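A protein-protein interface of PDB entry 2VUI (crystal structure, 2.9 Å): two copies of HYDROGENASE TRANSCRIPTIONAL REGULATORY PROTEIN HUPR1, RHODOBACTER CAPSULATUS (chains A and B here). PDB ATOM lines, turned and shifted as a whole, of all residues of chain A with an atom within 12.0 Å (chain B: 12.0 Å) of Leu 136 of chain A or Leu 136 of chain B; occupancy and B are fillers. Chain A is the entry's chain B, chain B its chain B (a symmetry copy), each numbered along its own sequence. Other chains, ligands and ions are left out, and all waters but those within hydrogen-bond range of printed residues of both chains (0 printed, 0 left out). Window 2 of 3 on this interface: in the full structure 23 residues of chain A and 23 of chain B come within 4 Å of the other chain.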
ATOM      1  N   GLU A 127     -36.931   6.156  -0.607  1.00  0.00           N
ATOM      2  CA  GLU A 127     -37.598   6.518  -1.852  1.00  0.00           C
ATOM      3  C   GLU A 127     -36.717   7.430  -2.683  1.00  0.00           C
ATOM      4  O   GLU A 127     -36.636   7.296  -3.907  1.00  0.00           O
ATOM      5  CB  GLU A 127     -38.926   7.224  -1.577  1.00  0.00           C
ATOM      6  CG  GLU A 127     -39.873   7.162  -2.777  1.00  0.00           C
ATOM      7  CD  GLU A 127     -40.777   8.379  -2.917  1.00  0.00           C
ATOM      8  OE1 GLU A 127     -40.661   9.328  -2.103  1.00  0.00           O
ATOM      9  OE2 GLU A 127     -41.602   8.380  -3.861  1.00  0.00           O
ATOM     10  N   ARG A 128     -36.084   8.378  -1.998  1.00  0.00           N
ATOM     11  CA  ARG A 128     -35.090   9.262  -2.593  1.00  0.00           C
ATOM     12  C   ARG A 128     -34.107   8.440  -3.425  1.00  0.00           C
ATOM     13  O   ARG A 128     -33.920   8.688  -4.612  1.00  0.00           O
ATOM     14  CB  ARG A 128     -34.360  10.014  -1.475  1.00  0.00           C
ATOM     15  CG  ARG A 128     -33.511  11.197  -1.904  1.00  0.00           C
ATOM     16  CD  ARG A 128     -33.082  11.978  -0.673  1.00  0.00           C
ATOM     17  NE  ARG A 128     -31.920  12.833  -0.898  1.00  0.00           N
ATOM     18  CZ  ARG A 128     -30.660  12.424  -0.783  1.00  0.00           C
ATOM     19  NH1 ARG A 128     -30.394  11.162  -0.464  1.00  0.00           N
ATOM     20  NH2 ARG A 128     -29.666  13.277  -0.996  1.00  0.00           N
ATOM     21  N   LEU A 129     -33.489   7.450  -2.798  1.00  0.00           N
ATOM     22  CA  LEU A 129     -32.594   6.551  -3.503  1.00  0.00           C
ATOM     23  C   LEU A 129     -33.226   6.091  -4.813  1.00  0.00           C
ATOM     24  O   LEU A 129     -32.648   6.267  -5.883  1.00  0.00           O
ATOM     25  CB  LEU A 129     -32.256   5.343  -2.626  1.00  0.00           C
ATOM     26  CG  LEU A 129     -31.665   5.631  -1.243  1.00  0.00           C
ATOM     27  CD1 LEU A 129     -31.450   4.353  -0.460  1.00  0.00           C
ATOM     28  CD2 LEU A 129     -30.365   6.396  -1.371  1.00  0.00           C
ATOM     29  N   SER A 130     -34.418   5.507  -4.721  1.00  0.00           N
ATOM     30  CA  SER A 130     -35.142   5.030  -5.893  1.00  0.00           C
ATOM     31  C   SER A 130     -35.252   6.115  -6.949  1.00  0.00           C
ATOM     32  O   SER A 130     -34.580   6.060  -7.976  1.00  0.00           O
ATOM     33  CB  SER A 130     -36.537   4.574  -5.498  1.00  0.00           C
ATOM     34  OG  SER A 130     -36.471   3.631  -4.450  1.00  0.00           O
ATOM     35  N   LEU A 131     -36.109   7.097  -6.694  1.00  0.00           N
ATOM     36  CA  LEU A 131     -36.267   8.221  -7.608  1.00  0.00           C
ATOM     37  C   LEU A 131     -34.946   8.577  -8.287  1.00  0.00           C
ATOM     38  O   LEU A 131     -34.878   8.677  -9.507  1.00  0.00           O
ATOM     39  CB  LEU A 131     -36.833   9.449  -6.874  1.00  0.00           C
ATOM     40  CG  LEU A 131     -38.251   9.362  -6.304  1.00  0.00           C
ATOM     41  CD1 LEU A 131     -38.770  10.735  -5.897  1.00  0.00           C
ATOM     42  CD2 LEU A 131     -39.178   8.719  -7.321  1.00  0.00           C
ATOM     43  N   GLU A 132     -33.894   8.747  -7.494  1.00  0.00           N
ATOM     44  CA  GLU A 132     -32.617   9.233  -8.008  1.00  0.00           C
ATOM     45  C   GLU A 132     -31.831   8.174  -8.767  1.00  0.00           C
ATOM     46  O   GLU A 132     -31.007   8.491  -9.620  1.00  0.00           O
ATOM     47  CB  GLU A 132     -31.768   9.838  -6.884  1.00  0.00           C
ATOM     48  CG  GLU A 132     -32.158  11.269  -6.535  1.00  0.00           C
ATOM     49  CD  GLU A 132     -31.074  12.013  -5.775  1.00  0.00           C
ATOM     50  OE1 GLU A 132     -30.278  11.357  -5.069  1.00  0.00           O
ATOM     51  OE2 GLU A 132     -31.020  13.258  -5.881  1.00  0.00           O
ATOM     52  N   MET A 133     -32.088   6.915  -8.458  1.00  0.00           N
ATOM     53  CA  MET A 133     -31.441   5.840  -9.172  1.00  0.00           C
ATOM     54  C   MET A 133     -32.236   5.478 -10.420  1.00  0.00           C
ATOM     55  O   MET A 133     -31.779   4.695 -11.247  1.00  0.00           O
ATOM     56  CB  MET A 133     -31.272   4.630  -8.268  1.00  0.00           C
ATOM     57  CG  MET A 133     -30.285   3.616  -8.802  1.00  0.00           C
ATOM     58  SD  MET A 133     -29.384   2.766  -7.496  1.00  0.00           S
ATOM     59  CE  MET A 133     -28.652   1.416  -8.411  1.00  0.00           C
ATOM     60  N   ARG A 134     -33.433   6.044 -10.548  1.00  0.00           N
ATOM     61  CA  ARG A 134     -34.223   5.904 -11.769  1.00  0.00           C
ATOM     62  C   ARG A 134     -33.681   6.875 -12.781  1.00  0.00           C
ATOM     63  O   ARG A 134     -33.560   6.567 -13.962  1.00  0.00           O
ATOM     64  CB  ARG A 134     -35.695   6.253 -11.532  1.00  0.00           C
ATOM     65  CG  ARG A 134     -36.558   5.116 -11.022  1.00  0.00           C
ATOM     66  CD  ARG A 134     -38.025   5.524 -10.959  1.00  0.00           C
ATOM     67  NE  ARG A 134     -38.713   4.862  -9.856  1.00  0.00           N
ATOM     68  CZ  ARG A 134     -39.990   5.055  -9.537  1.00  0.00           C
ATOM     69  NH1 ARG A 134     -40.732   5.893 -10.247  1.00  0.00           N
ATOM     70  NH2 ARG A 134     -40.523   4.407  -8.506  1.00  0.00           N
ATOM     71  N   LEU A 135     -33.366   8.067 -12.301  1.00  0.00           N
ATOM     72  CA  LEU A 135     -32.858   9.115 -13.156  1.00  0.00           C
ATOM     73  C   LEU A 135     -31.436   8.796 -13.608  1.00  0.00           C
ATOM     74  O   LEU A 135     -30.623   9.692 -13.826  1.00  0.00           O
ATOM     75  CB  LEU A 135     -32.920  10.456 -12.431  1.00  0.00           C
ATOM     76  CG  LEU A 135     -34.333  10.937 -12.098  1.00  0.00           C
ATOM     77  CD1 LEU A 135     -34.292  12.319 -11.476  1.00  0.00           C
ATOM     78  CD2 LEU A 135     -35.200  10.934 -13.342  1.00  0.00           C
ATOM     79  N   LEU A 136     -31.147   7.509 -13.756  1.00  0.00           N
ATOM     80  CA  LEU A 136     -29.851   7.066 -14.250  1.00  0.00           C
ATOM     81  C   LEU A 136     -30.009   6.115 -15.426  1.00  0.00           C
ATOM     82  O   LEU A 136     -29.479   6.364 -16.509  1.00  0.00           O
ATOM     83  CB  LEU A 136     -29.063   6.397 -13.131  1.00  0.00           C
ATOM     84  CG  LEU A 136     -28.991   7.235 -11.851  1.00  0.00           C
ATOM     85  CD1 LEU A 136     -28.274   6.482 -10.741  1.00  0.00           C
ATOM     86  CD2 LEU A 136     -28.324   8.576 -12.121  1.00  0.00           C
ATOM     87  N   GLU A 137     -30.741   5.026 -15.211  1.00  0.00           N
ATOM     88  CA  GLU A 137     -30.987   4.055 -16.272  1.00  0.00           C
ATOM     89  C   GLU A 137     -31.832   4.655 -17.394  1.00  0.00           C
ATOM     90  O   GLU A 137     -31.316   5.346 -18.275  1.00  0.00           O
ATOM     91  CB  GLU A 137     -31.657   2.811 -15.712  1.00  0.00           C
ATOM     92  N   GLU B 127     -30.273  -0.162   2.101  1.00  0.00           N
ATOM     93  CA  GLU B 127     -28.827  -0.291   1.972  1.00  0.00           C
ATOM     94  C   GLU B 127     -28.458  -0.829   0.604  1.00  0.00           C
ATOM     95  O   GLU B 127     -27.492  -0.383  -0.018  1.00  0.00           O
ATOM     96  CB  GLU B 127     -28.263  -1.226   3.043  1.00  0.00           C
ATOM     97  CG  GLU B 127     -26.768  -0.999   3.278  1.00  0.00           C
ATOM     98  CD  GLU B 127     -26.003  -2.258   3.666  1.00  0.00           C
ATOM     99  OE1 GLU B 127     -26.613  -3.355   3.720  1.00  0.00           O
ATOM    100  OE2 GLU B 127     -24.778  -2.140   3.905  1.00  0.00           O
ATOM    101  N   ARG B 128     -29.230  -1.819   0.163  1.00  0.00           N
ATOM    102  CA  ARG B 128     -29.125  -2.375  -1.181  1.00  0.00           C
ATOM    103  C   ARG B 128     -29.056  -1.238  -2.200  1.00  0.00           C
ATOM    104  O   ARG B 128     -28.121  -1.151  -2.989  1.00  0.00           O
ATOM    105  CB  ARG B 128     -30.338  -3.271  -1.446  1.00  0.00           C
ATOM    106  CG  ARG B 128     -30.253  -4.174  -2.662  1.00  0.00           C
ATOM    107  CD  ARG B 128     -31.401  -5.170  -2.629  1.00  0.00           C
ATOM    108  NE  ARG B 128     -31.697  -5.767  -3.927  1.00  0.00           N
ATOM    109  CZ  ARG B 128     -32.511  -5.224  -4.828  1.00  0.00           C
ATOM    110  NH1 ARG B 128     -33.097  -4.058  -4.581  1.00  0.00           N
ATOM    111  NH2 ARG B 128     -32.730  -5.846  -5.980  1.00  0.00           N
ATOM    112  N   LEU B 129     -30.047  -0.359  -2.170  1.00  0.00           N
ATOM    113  CA  LEU B 129     -30.051   0.805  -3.034  1.00  0.00           C
ATOM    114  C   LEU B 129     -28.685   1.485  -3.016  1.00  0.00           C
ATOM    115  O   LEU B 129     -28.063   1.667  -4.060  1.00  0.00           O
ATOM    116  CB  LEU B 129     -31.137   1.790  -2.594  1.00  0.00           C
ATOM    117  CG  LEU B 129     -32.567   1.251  -2.498  1.00  0.00           C
ATOM    118  CD1 LEU B 129     -33.520   2.309  -1.981  1.00  0.00           C
ATOM    119  CD2 LEU B 129     -33.031   0.736  -3.845  1.00  0.00           C
ATOM    120  N   SER B 130     -28.223   1.851  -1.824  1.00  0.00           N
ATOM    121  CA  SER B 130     -26.927   2.499  -1.659  1.00  0.00           C
ATOM    122  C   SER B 130     -25.828   1.710  -2.346  1.00  0.00           C
ATOM    123  O   SER B 130     -25.323   2.116  -3.390  1.00  0.00           O
ATOM    124  CB  SER B 130     -26.594   2.637  -0.182  1.00  0.00           C
ATOM    125  OG  SER B 130     -27.644   3.286   0.503  1.00  0.00           O
ATOM    126  N   LEU B 131     -25.454   0.583  -1.750  1.00  0.00           N
ATOM    127  CA  LEU B 131     -24.442  -0.286  -2.339  1.00  0.00           C
ATOM    128  C   LEU B 131     -24.512  -0.268  -3.865  1.00  0.00           C
ATOM    129  O   LEU B 131     -23.509  -0.047  -4.532  1.00  0.00           O
ATOM    130  CB  LEU B 131     -24.588  -1.726  -1.819  1.00  0.00           C
ATOM    131  CG  LEU B 131     -24.339  -1.989  -0.331  1.00  0.00           C
ATOM    132  CD1 LEU B 131     -24.213  -3.479  -0.046  1.00  0.00           C
ATOM    133  CD2 LEU B 131     -23.090  -1.250   0.120  1.00  0.00           C
ATOM    134  N   GLU B 132     -25.705  -0.480  -4.410  1.00  0.00           N
ATOM    135  CA  GLU B 132     -25.870  -0.633  -5.852  1.00  0.00           C
ATOM    136  C   GLU B 132     -25.795   0.683  -6.611  1.00  0.00           C
ATOM    137  O   GLU B 132     -25.464   0.711  -7.793  1.00  0.00           O
ATOM    138  CB  GLU B 132     -27.173  -1.374  -6.178  1.00  0.00           C
ATOM    139  CG  GLU B 132     -27.059  -2.888  -6.042  1.00  0.00           C
ATOM    140  CD  GLU B 132     -28.158  -3.636  -6.774  1.00  0.00           C
ATOM    141  OE1 GLU B 132     -29.261  -3.072  -6.939  1.00  0.00           O
ATOM    142  OE2 GLU B 132     -27.919  -4.793  -7.184  1.00  0.00           O
ATOM    143  N   MET B 133     -26.100   1.774  -5.931  1.00  0.00           N
ATOM    144  CA  MET B 133     -25.991   3.075  -6.547  1.00  0.00           C
ATOM    145  C   MET B 133     -24.578   3.621  -6.388  1.00  0.00           C
ATOM    146  O   MET B 133     -24.234   4.645  -6.972  1.00  0.00           O
ATOM    147  CB  MET B 133     -27.012   4.030  -5.951  1.00  0.00           C
ATOM    148  CG  MET B 133     -27.224   5.276  -6.783  1.00  0.00           C
ATOM    149  SD  MET B 133     -28.914   5.890  -6.698  1.00  0.00           S
ATOM    150  CE  MET B 133     -28.720   7.517  -7.414  1.00  0.00           C
ATOM    151  N   ARG B 134     -23.764   2.941  -5.586  1.00  0.00           N
ATOM    152  CA  ARG B 134     -22.345   3.269  -5.472  1.00  0.00           C
ATOM    153  C   ARG B 134     -21.640   2.671  -6.658  1.00  0.00           C
ATOM    154  O   ARG B 134     -20.754   3.279  -7.250  1.00  0.00           O
ATOM    155  CB  ARG B 134     -21.724   2.666  -4.209  1.00  0.00           C
ATOM    156  CG  ARG B 134     -21.864   3.503  -2.954  1.00  0.00           C
ATOM    157  CD  ARG B 134     -21.092   2.887  -1.794  1.00  0.00           C
ATOM    158  NE  ARG B 134     -21.754   3.146  -0.518  1.00  0.00           N
ATOM    159  CZ  ARG B 134     -21.326   2.699   0.659  1.00  0.00           C
ATOM    160  NH1 ARG B 134     -20.222   1.969   0.731  1.00  0.00           N
ATOM    161  NH2 ARG B 134     -22.006   2.985   1.764  1.00  0.00           N
ATOM    162  N   LEU B 135     -22.038   1.454  -6.991  1.00  0.00           N
ATOM    163  CA  LEU B 135     -21.436   0.738  -8.093  1.00  0.00           C
ATOM    164  C   LEU B 135     -21.845   1.359  -9.424  1.00  0.00           C
ATOM    165  O   LEU B 135     -21.959   0.672 -10.438  1.00  0.00           O
ATOM    166  CB  LEU B 135     -21.821  -0.737  -8.029  1.00  0.00           C
ATOM    167  CG  LEU B 135     -21.294  -1.482  -6.802  1.00  0.00           C
ATOM    168  CD1 LEU B 135     -21.641  -2.956  -6.886  1.00  0.00           C
ATOM    169  CD2 LEU B 135     -19.795  -1.291  -6.670  1.00  0.00           C
ATOM    170  N   LEU B 136     -22.055   2.670  -9.415  1.00  0.00           N
ATOM    171  CA  LEU B 136     -22.380   3.403 -10.631  1.00  0.00           C
ATOM    172  C   LEU B 136     -21.445   4.587 -10.823  1.00  0.00           C
ATOM    173  O   LEU B 136     -20.777   4.695 -11.851  1.00  0.00           O
ATOM    174  CB  LEU B 136     -23.828   3.875 -10.588  1.00  0.00           C
ATOM    175  CG  LEU B 136     -24.822   2.761 -10.244  1.00  0.00           C
ATOM    176  CD1 LEU B 136     -26.237   3.307 -10.124  1.00  0.00           C
ATOM    177  CD2 LEU B 136     -24.753   1.641 -11.270  1.00  0.00           C
ATOM    178  N   GLU B 137     -21.398   5.470  -9.832  1.00  0.00           N
ATOM    179  CA  GLU B 137     -20.516   6.632  -9.890  1.00  0.00           C
ATOM    180  C   GLU B 137     -19.046   6.218  -9.870  1.00  0.00           C
ATOM    181  O   GLU B 137     -18.477   5.852 -10.901  1.00  0.00           O
ATOM    182  CB  GLU B 137     -20.814   7.586  -8.747  1.00  0.00           C
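Among the printed residues, merely in contact across the chains: Leu 129 of chain A with Leu 129 of chain B, Met 133 of chain A with Glu 132 of chain B, Glu 132 of chain A with Met 133 of chain B, Leu 136 of chain A with Met 133 of chain B, Met 133 of chain A with Leu 136 of chain B, Leu 136 of chain A with Leu 136 of chain B, Leu 129 of chain A with Met 133 of chain B and Met 133 of chain A with Leu 129 of chain B.
Printed residues of chain A that touch a printed residue of chain B: Leu 129, Glu 132, Met 133 and Leu 136.
Hydrophobic or aromatic side chains of chain A that line the printed part of chain B: Leu 129, Met 133 and Leu 136.
Among the printed residues, 9 pairs touch across the chains.
Among the printed residues, no Asp or Glu carboxylate lies within 4 Å of a Lys or Arg side-chain nitrogen of the other chain.
Leu 129 of chain A touches Met 133 of chain B, and with the chains exchanged Met 133 of chain A touches Leu 129 of chain B.
Met 133 of chain A touches its own counterpart, Met 133 of chain B.
Met 133 of chain A touches Leu 136 of chain B, and with the chains exchanged Leu 136 of chain A touches Met 133 of chain B.
Leu 136 of chain B touches its own counterpart, Leu 136 of chain A.
Of the 9 pairs that touch across the chains among the printed residues, 9 have their exchanged pair printed and touching as well.
The backbone NH (N) of Met 133 of chain A sits close to the side-chain sulfur (SD) of Met 133 of chain B (3.8 Å).
Glu 127 of chain A touches none of the printed residues of chain B.
Printed residues of chain B within 4 Å of Leu 129 of chain A: Leu 129 and Met 133.
Printed residues of chain B within 4 Å of Glu 132 of chain A: Met 133 (3.3 Å).
Of the printed residues of chain B, Met 133 of chain A touches Leu 129 (3.8 Å), Glu 132 (3.3 Å), Met 133 (3.1 Å) and Leu 136 (3.5 Å).
Of chain B, only Met 133 (3.5 Å) and Leu 136 (3.8 Å) come within 4 Å of Leu 136 of chain A.
No residue of chain B comes within 4 Å of Glu 137 of chain A.
Glu 127 of chain B touches none of the printed residues of chain A.
Of the printed residues of chain A, Leu 129 of chain B touches Leu 129 and Met 133.
Of the printed residues of chain A, Glu 132 of chain B touches Met 133 (3.3 Å).
Of chain A, only Leu 129, Glu 132, Met 133 and Leu 136 come within 4 Å of Met 133 of chain B.
No residue of chain A comes within 4 Å of Leu 135 of chain B.
Leu 136 of chain B touches two residues of chain A.
No residue of chain A comes within 4 Å of Glu 137 of chain B.
The nearest printed residue of chain A that does not touch Glu 132 of chain B is Leu 136 of chain A (7.1 Å).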
